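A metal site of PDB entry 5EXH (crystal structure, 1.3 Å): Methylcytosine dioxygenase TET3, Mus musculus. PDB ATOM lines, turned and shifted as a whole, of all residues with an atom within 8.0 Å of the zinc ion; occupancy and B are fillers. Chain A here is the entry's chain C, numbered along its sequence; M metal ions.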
ATOM      1  N   ARG A  16     -21.369 -14.061   2.088  1.00  0.00           N
ATOM      2  CA  ARG A  16     -20.048 -14.195   1.461  1.00  0.00           C
ATOM      3  C   ARG A  16     -19.283 -12.885   1.496  1.00  0.00           C
ATOM      4  O   ARG A  16     -19.845 -11.808   1.308  1.00  0.00           O
ATOM      5  CB  ARG A  16     -20.179 -14.650   0.008  1.00  0.00           C
ATOM      6  CG  ARG A  16     -20.644 -16.069  -0.155  1.00  0.00           C
ATOM      7  CD  ARG A  16     -20.490 -16.529  -1.599  1.00  0.00           C
ATOM      8  NE  ARG A  16     -19.137 -16.997  -1.894  1.00  0.00           N
ATOM      9  CZ  ARG A  16     -18.692 -18.220  -1.598  1.00  0.00           C
ATOM     10  NH1 ARG A  16     -19.503 -19.072  -0.979  1.00  0.00           N
ATOM     11  NH2 ARG A  16     -17.455 -18.573  -1.896  1.00  0.00           N
ATOM     12  N   GLU A  18     -16.430 -12.021  -0.329  1.00  0.00           N
ATOM     13  CA  GLU A  18     -15.717 -11.591  -1.527  1.00  0.00           C
ATOM     14  C   GLU A  18     -16.403 -12.072  -2.789  1.00  0.00           C
ATOM     15  O   GLU A  18     -17.099 -13.082  -2.793  1.00  0.00           O
ATOM     16  CB  GLU A  18     -14.276 -12.127  -1.492  1.00  0.00           C
ATOM     17  CG  GLU A  18     -13.555 -11.933  -0.168  1.00  0.00           C
ATOM     18  CD  GLU A  18     -12.053 -12.029  -0.292  1.00  0.00           C
ATOM     19  OE1 GLU A  18     -11.566 -12.568  -1.309  1.00  0.00           O
ATOM     20  OE2 GLU A  18     -11.359 -11.561   0.631  1.00  0.00           O
ATOM     21  N   ASN A  19     -16.198 -11.327  -3.884  1.00  0.00           N
ATOM     22  CA  ASN A  19     -16.557 -11.841  -5.197  1.00  0.00           C
ATOM     23  C   ASN A  19     -15.753 -13.102  -5.496  1.00  0.00           C
ATOM     24  O   ASN A  19     -14.566 -13.181  -5.156  1.00  0.00           O
ATOM     25  CB  ASN A  19     -16.287 -10.789  -6.266  1.00  0.00           C
ATOM     26  CG  ASN A  19     -17.217  -9.604  -6.163  1.00  0.00           C
ATOM     27  OD1 ASN A  19     -18.401  -9.760  -5.910  1.00  0.00           O
ATOM     28  ND2 ASN A  19     -16.671  -8.405  -6.361  1.00  0.00           N
ATOM     29  N   CYS A  20     -16.378 -14.085  -6.138  1.00  0.00           N
ATOM     30  CA  CYS A  20     -15.709 -15.374  -6.346  1.00  0.00           C
ATOM     31  C   CYS A  20     -14.577 -15.292  -7.373  1.00  0.00           C
ATOM     32  O   CYS A  20     -13.641 -16.098  -7.332  1.00  0.00           O
ATOM     33  CB  CYS A  20     -16.697 -16.491  -6.719  1.00  0.00           C
ATOM     34  SG  CYS A  20     -17.326 -16.484  -8.424  1.00  0.00           S
ATOM     35  N   GLY A  21     -14.679 -14.338  -8.292  1.00  0.00           N
ATOM     36  CA  GLY A  21     -13.639 -14.114  -9.269  1.00  0.00           C
ATOM     37  C   GLY A  21     -13.684 -14.991 -10.505  1.00  0.00           C
ATOM     38  O   GLY A  21     -12.901 -14.777 -11.443  1.00  0.00           O
ATOM     39  N   SER A  22     -14.594 -15.968 -10.549  1.00  0.00           N
ATOM     40  CA  SER A  22     -14.593 -16.887 -11.691  1.00  0.00           C
ATOM     41  C   SER A  22     -15.956 -17.187 -12.323  1.00  0.00           C
ATOM     42  O   SER A  22     -16.007 -17.758 -13.406  1.00  0.00           O
ATOM     43  CB  SER A  22     -13.880 -18.185 -11.327  1.00  0.00           C
ATOM     44  OG  SER A  22     -14.556 -18.833 -10.268  1.00  0.00           O
ATOM     45  N   CYS A  23     -17.054 -16.811 -11.659  1.00  0.00           N
ATOM     46  CA  CYS A  23     -18.372 -17.014 -12.259  1.00  0.00           C
ATOM     47  C   CYS A  23     -18.575 -16.074 -13.452  1.00  0.00           C
ATOM     48  O   CYS A  23     -17.753 -15.190 -13.723  1.00  0.00           O
ATOM     49  CB  CYS A  23     -19.471 -16.779 -11.220  1.00  0.00           C
ATOM     50  SG  CYS A  23     -19.756 -15.055 -10.829  1.00  0.00           S
ATOM     51  N   THR A  24     -19.695 -16.259 -14.141  1.00  0.00           N
ATOM     52  CA  THR A  24     -19.984 -15.439 -15.317  1.00  0.00           C
ATOM     53  C   THR A  24     -19.985 -13.940 -14.983  1.00  0.00           C
ATOM     54  O   THR A  24     -19.436 -13.128 -15.733  1.00  0.00           O
ATOM     55  CB  THR A  24     -21.316 -15.820 -15.952  1.00  0.00           C
ATOM     56  OG1 THR A  24     -21.481 -17.248 -15.910  1.00  0.00           O
ATOM     57  CG2 THR A  24     -21.384 -15.312 -17.379  1.00  0.00           C
ATOM     58  N   SER A  25     -20.599 -13.564 -13.871  1.00  0.00           N
ATOM     59  CA  SER A  25     -20.670 -12.152 -13.510  1.00  0.00           C
ATOM     60  C   SER A  25     -19.295 -11.580 -13.165  1.00  0.00           C
ATOM     61  O   SER A  25     -19.012 -10.412 -13.462  1.00  0.00           O
ATOM     62  CB  SER A  25     -21.600 -11.941 -12.317  1.00  0.00           C
ATOM     63  OG  SER A  25     -22.917 -12.311 -12.639  1.00  0.00           O
ATOM     64  N   CYS A  26     -18.458 -12.396 -12.535  1.00  0.00           N
ATOM     65  CA  CYS A  26     -17.105 -11.985 -12.173  1.00  0.00           C
ATOM     66  C   CYS A  26     -16.159 -12.003 -13.370  1.00  0.00           C
ATOM     67  O   CYS A  26     -15.043 -11.481 -13.291  1.00  0.00           O
ATOM     68  CB  CYS A  26     -16.537 -12.887 -11.067  1.00  0.00           C
ATOM     69  SG  CYS A  26     -17.268 -12.600  -9.454  1.00  0.00           S
ATOM     70  N   THR A  27     -16.605 -12.599 -14.477  1.00  0.00           N
ATOM     71  CA  THR A  27     -15.772 -12.866 -15.651  1.00  0.00           C
ATOM     72  C   THR A  27     -16.098 -11.909 -16.818  1.00  0.00           C
ATOM     73  O   THR A  27     -15.209 -11.312 -17.433  1.00  0.00           O
ATOM     74  CB  THR A  27     -15.921 -14.345 -16.126  1.00  0.00           C
ATOM     75  OG1 THR A  27     -15.502 -15.221 -15.074  1.00  0.00           O
ATOM     76  CG2 THR A  27     -15.052 -14.607 -17.348  1.00  0.00           C
ATOM     77  N   GLN A  33     -24.009  -7.188 -13.415  1.00  0.00           N
ATOM     78  CA  GLN A  33     -24.666  -8.135 -12.529  1.00  0.00           C
ATOM     79  C   GLN A  33     -23.727  -8.573 -11.403  1.00  0.00           C
ATOM     80  O   GLN A  33     -22.534  -8.765 -11.633  1.00  0.00           O
ATOM     81  CB  GLN A  33     -25.132  -9.329 -13.341  1.00  0.00           C
ATOM     82  CG  GLN A  33     -26.033 -10.317 -12.627  1.00  0.00           C
ATOM     83  CD  GLN A  33     -26.639 -11.298 -13.596  1.00  0.00           C
ATOM     84  OE1 GLN A  33     -27.114 -10.918 -14.665  1.00  0.00           O
ATOM     85  NE2 GLN A  33     -26.602 -12.574 -13.249  1.00  0.00           N
ATOM     86  N   ILE A  34     -24.273  -8.736 -10.197  1.00  0.00           N
ATOM     87  CA  ILE A  34     -23.480  -9.192  -9.052  1.00  0.00           C
ATOM     88  C   ILE A  34     -22.991 -10.630  -9.248  1.00  0.00           C
ATOM     89  O   ILE A  34     -23.633 -11.426  -9.949  1.00  0.00           O
ATOM     90  CB  ILE A  34     -24.304  -9.093  -7.742  1.00  0.00           C
ATOM     91  CG1 ILE A  34     -23.402  -9.105  -6.505  1.00  0.00           C
ATOM     92  CG2 ILE A  34     -25.359 -10.186  -7.687  1.00  0.00           C
ATOM     93  CD1 ILE A  34     -24.162  -8.980  -5.185  1.00  0.00           C
ATOM     94  N   CYS A  35     -21.831 -10.935  -8.643  1.00  0.00           N
ATOM     95  CA  CYS A  35     -21.305 -12.290  -8.547  1.00  0.00           C
ATOM     96  C   CYS A  35     -22.441 -13.282  -8.294  1.00  0.00           C
ATOM     97  O   CYS A  35     -23.246 -13.096  -7.394  1.00  0.00           O
ATOM     98  CB  CYS A  35     -20.292 -12.363  -7.403  1.00  0.00           C
ATOM     99  SG  CYS A  35     -19.699 -14.008  -6.989  1.00  0.00           S
ATOM    100  N   LYS A  36     -22.494 -14.337  -9.100  1.00  0.00           N
ATOM    101  CA  LYS A  36     -23.557 -15.320  -8.965  1.00  0.00           C
ATOM    102  C   LYS A  36     -23.591 -15.954  -7.591  1.00  0.00           C
ATOM    103  O   LYS A  36     -24.665 -16.292  -7.088  1.00  0.00           O
ATOM    104  CB  LYS A  36     -23.434 -16.394 -10.047  1.00  0.00           C
ATOM    105  CG  LYS A  36     -23.605 -15.819 -11.440  1.00  0.00           C
ATOM    106  CD  LYS A  36     -23.700 -16.880 -12.507  1.00  0.00           C
ATOM    107  CE  LYS A  36     -24.150 -16.248 -13.823  1.00  0.00           C
ATOM    108  NZ  LYS A  36     -24.139 -17.234 -14.950  1.00  0.00           N
ATOM    109  N   LEU A  37     -22.433 -16.091  -6.969  1.00  0.00           N
ATOM    110  CA  LEU A  37     -22.343 -16.727  -5.660  1.00  0.00           C
ATOM    111  C   LEU A  37     -22.787 -15.790  -4.532  1.00  0.00           C
ATOM    112  O   LEU A  37     -23.062 -16.237  -3.411  1.00  0.00           O
ATOM    113  CB  LEU A  37     -20.927 -17.247  -5.403  1.00  0.00           C
ATOM    114  CG  LEU A  37     -20.566 -18.574  -6.087  1.00  0.00           C
ATOM    115  CD1 LEU A  37     -21.424 -19.688  -5.547  1.00  0.00           C
ATOM    116  CD2 LEU A  37     -20.681 -18.558  -7.614  1.00  0.00           C
ATOM    117  N   ARG A  38     -22.896 -14.498  -4.845  1.00  0.00           N
ATOM    118  CA  ARG A  38     -23.314 -13.494  -3.865  1.00  0.00           C
ATOM    119  C   ARG A  38     -24.767 -13.048  -4.032  1.00  0.00           C
ATOM    120  O   ARG A  38     -25.320 -12.415  -3.136  1.00  0.00           O
ATOM    121  CB  ARG A  38     -22.382 -12.270  -3.896  1.00  0.00           C
ATOM    122  CG  ARG A  38     -20.948 -12.572  -3.456  1.00  0.00           C
ATOM    123  CD  ARG A  38     -20.098 -11.318  -3.384  1.00  0.00           C
ATOM    124  NE  ARG A  38     -20.816 -10.284  -2.639  1.00  0.00           N
ATOM    125  CZ  ARG A  38     -20.955  -9.018  -3.018  1.00  0.00           C
ATOM    126  NH1 ARG A  38     -20.373  -8.576  -4.132  1.00  0.00           N
ATOM    127  NH2 ARG A  38     -21.679  -8.199  -2.267  1.00  0.00           N
ATOM    128  N   LYS A  39     -25.397 -13.356  -5.170  1.00  0.00           N
ATOM    129  CA  LYS A  39     -26.745 -12.854  -5.420  1.00  0.00           C
ATOM    130  C   LYS A  39     -27.706 -13.313  -4.314  1.00  0.00           C
ATOM    131  O   LYS A  39     -27.798 -14.517  -4.036  1.00  0.00           O
ATOM    132  CB  LYS A  39     -27.249 -13.326  -6.789  1.00  0.00           C
ATOM    133  CG  LYS A  39     -28.688 -12.889  -7.118  1.00  0.00           C
ATOM    134  CD  LYS A  39     -28.814 -11.384  -7.357  1.00  0.00           C
ATOM    135  CE  LYS A  39     -30.247 -10.963  -7.636  1.00  0.00           C
ATOM    136  NZ  LYS A  39     -30.368  -9.538  -8.068  1.00  0.00           N
HETATM  137 ZN    ZN M   1     -18.500 -14.559  -8.908  1.00  0.00          ZN
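N of Lys 36 lies close to SG of Cys 23, at 3.3 Å. The side-chain sulfur of Cys 20 sits close to the backbone NH of Ser 22 (3.5 Å). The backbone NH of Gly 21 lies close to the side-chain sulfur of Cys 26, 3.3 Å away. SG of Cys 23 lies close to N of Ser 25, 3.5 Å away. OG1 of Thr 27 lies within hydrogen-bond range of O of Cys 23 (2.6 Å). The side-chain sulfur (SG) of Cys 35 lies close to the backbone NH (N) of Leu 37 (3.4 Å).
Gly 21 touches the zinc ion. Of the 18 residues printed, 5 come within 4 Å of the zinc ion. The nearest printed residue that does not touch the zinc ion is Lys 36 (4.005 Å).
The zinc ion is bound by the side-chain sulfur of Cys 20 (2.3 Å), the side-chain sulfur of Cys 35 (2.3 Å), the side-chain sulfur of Cys 23 (2.3 Å) and the side-chain sulfur of Cys 26 (2.4 Å).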
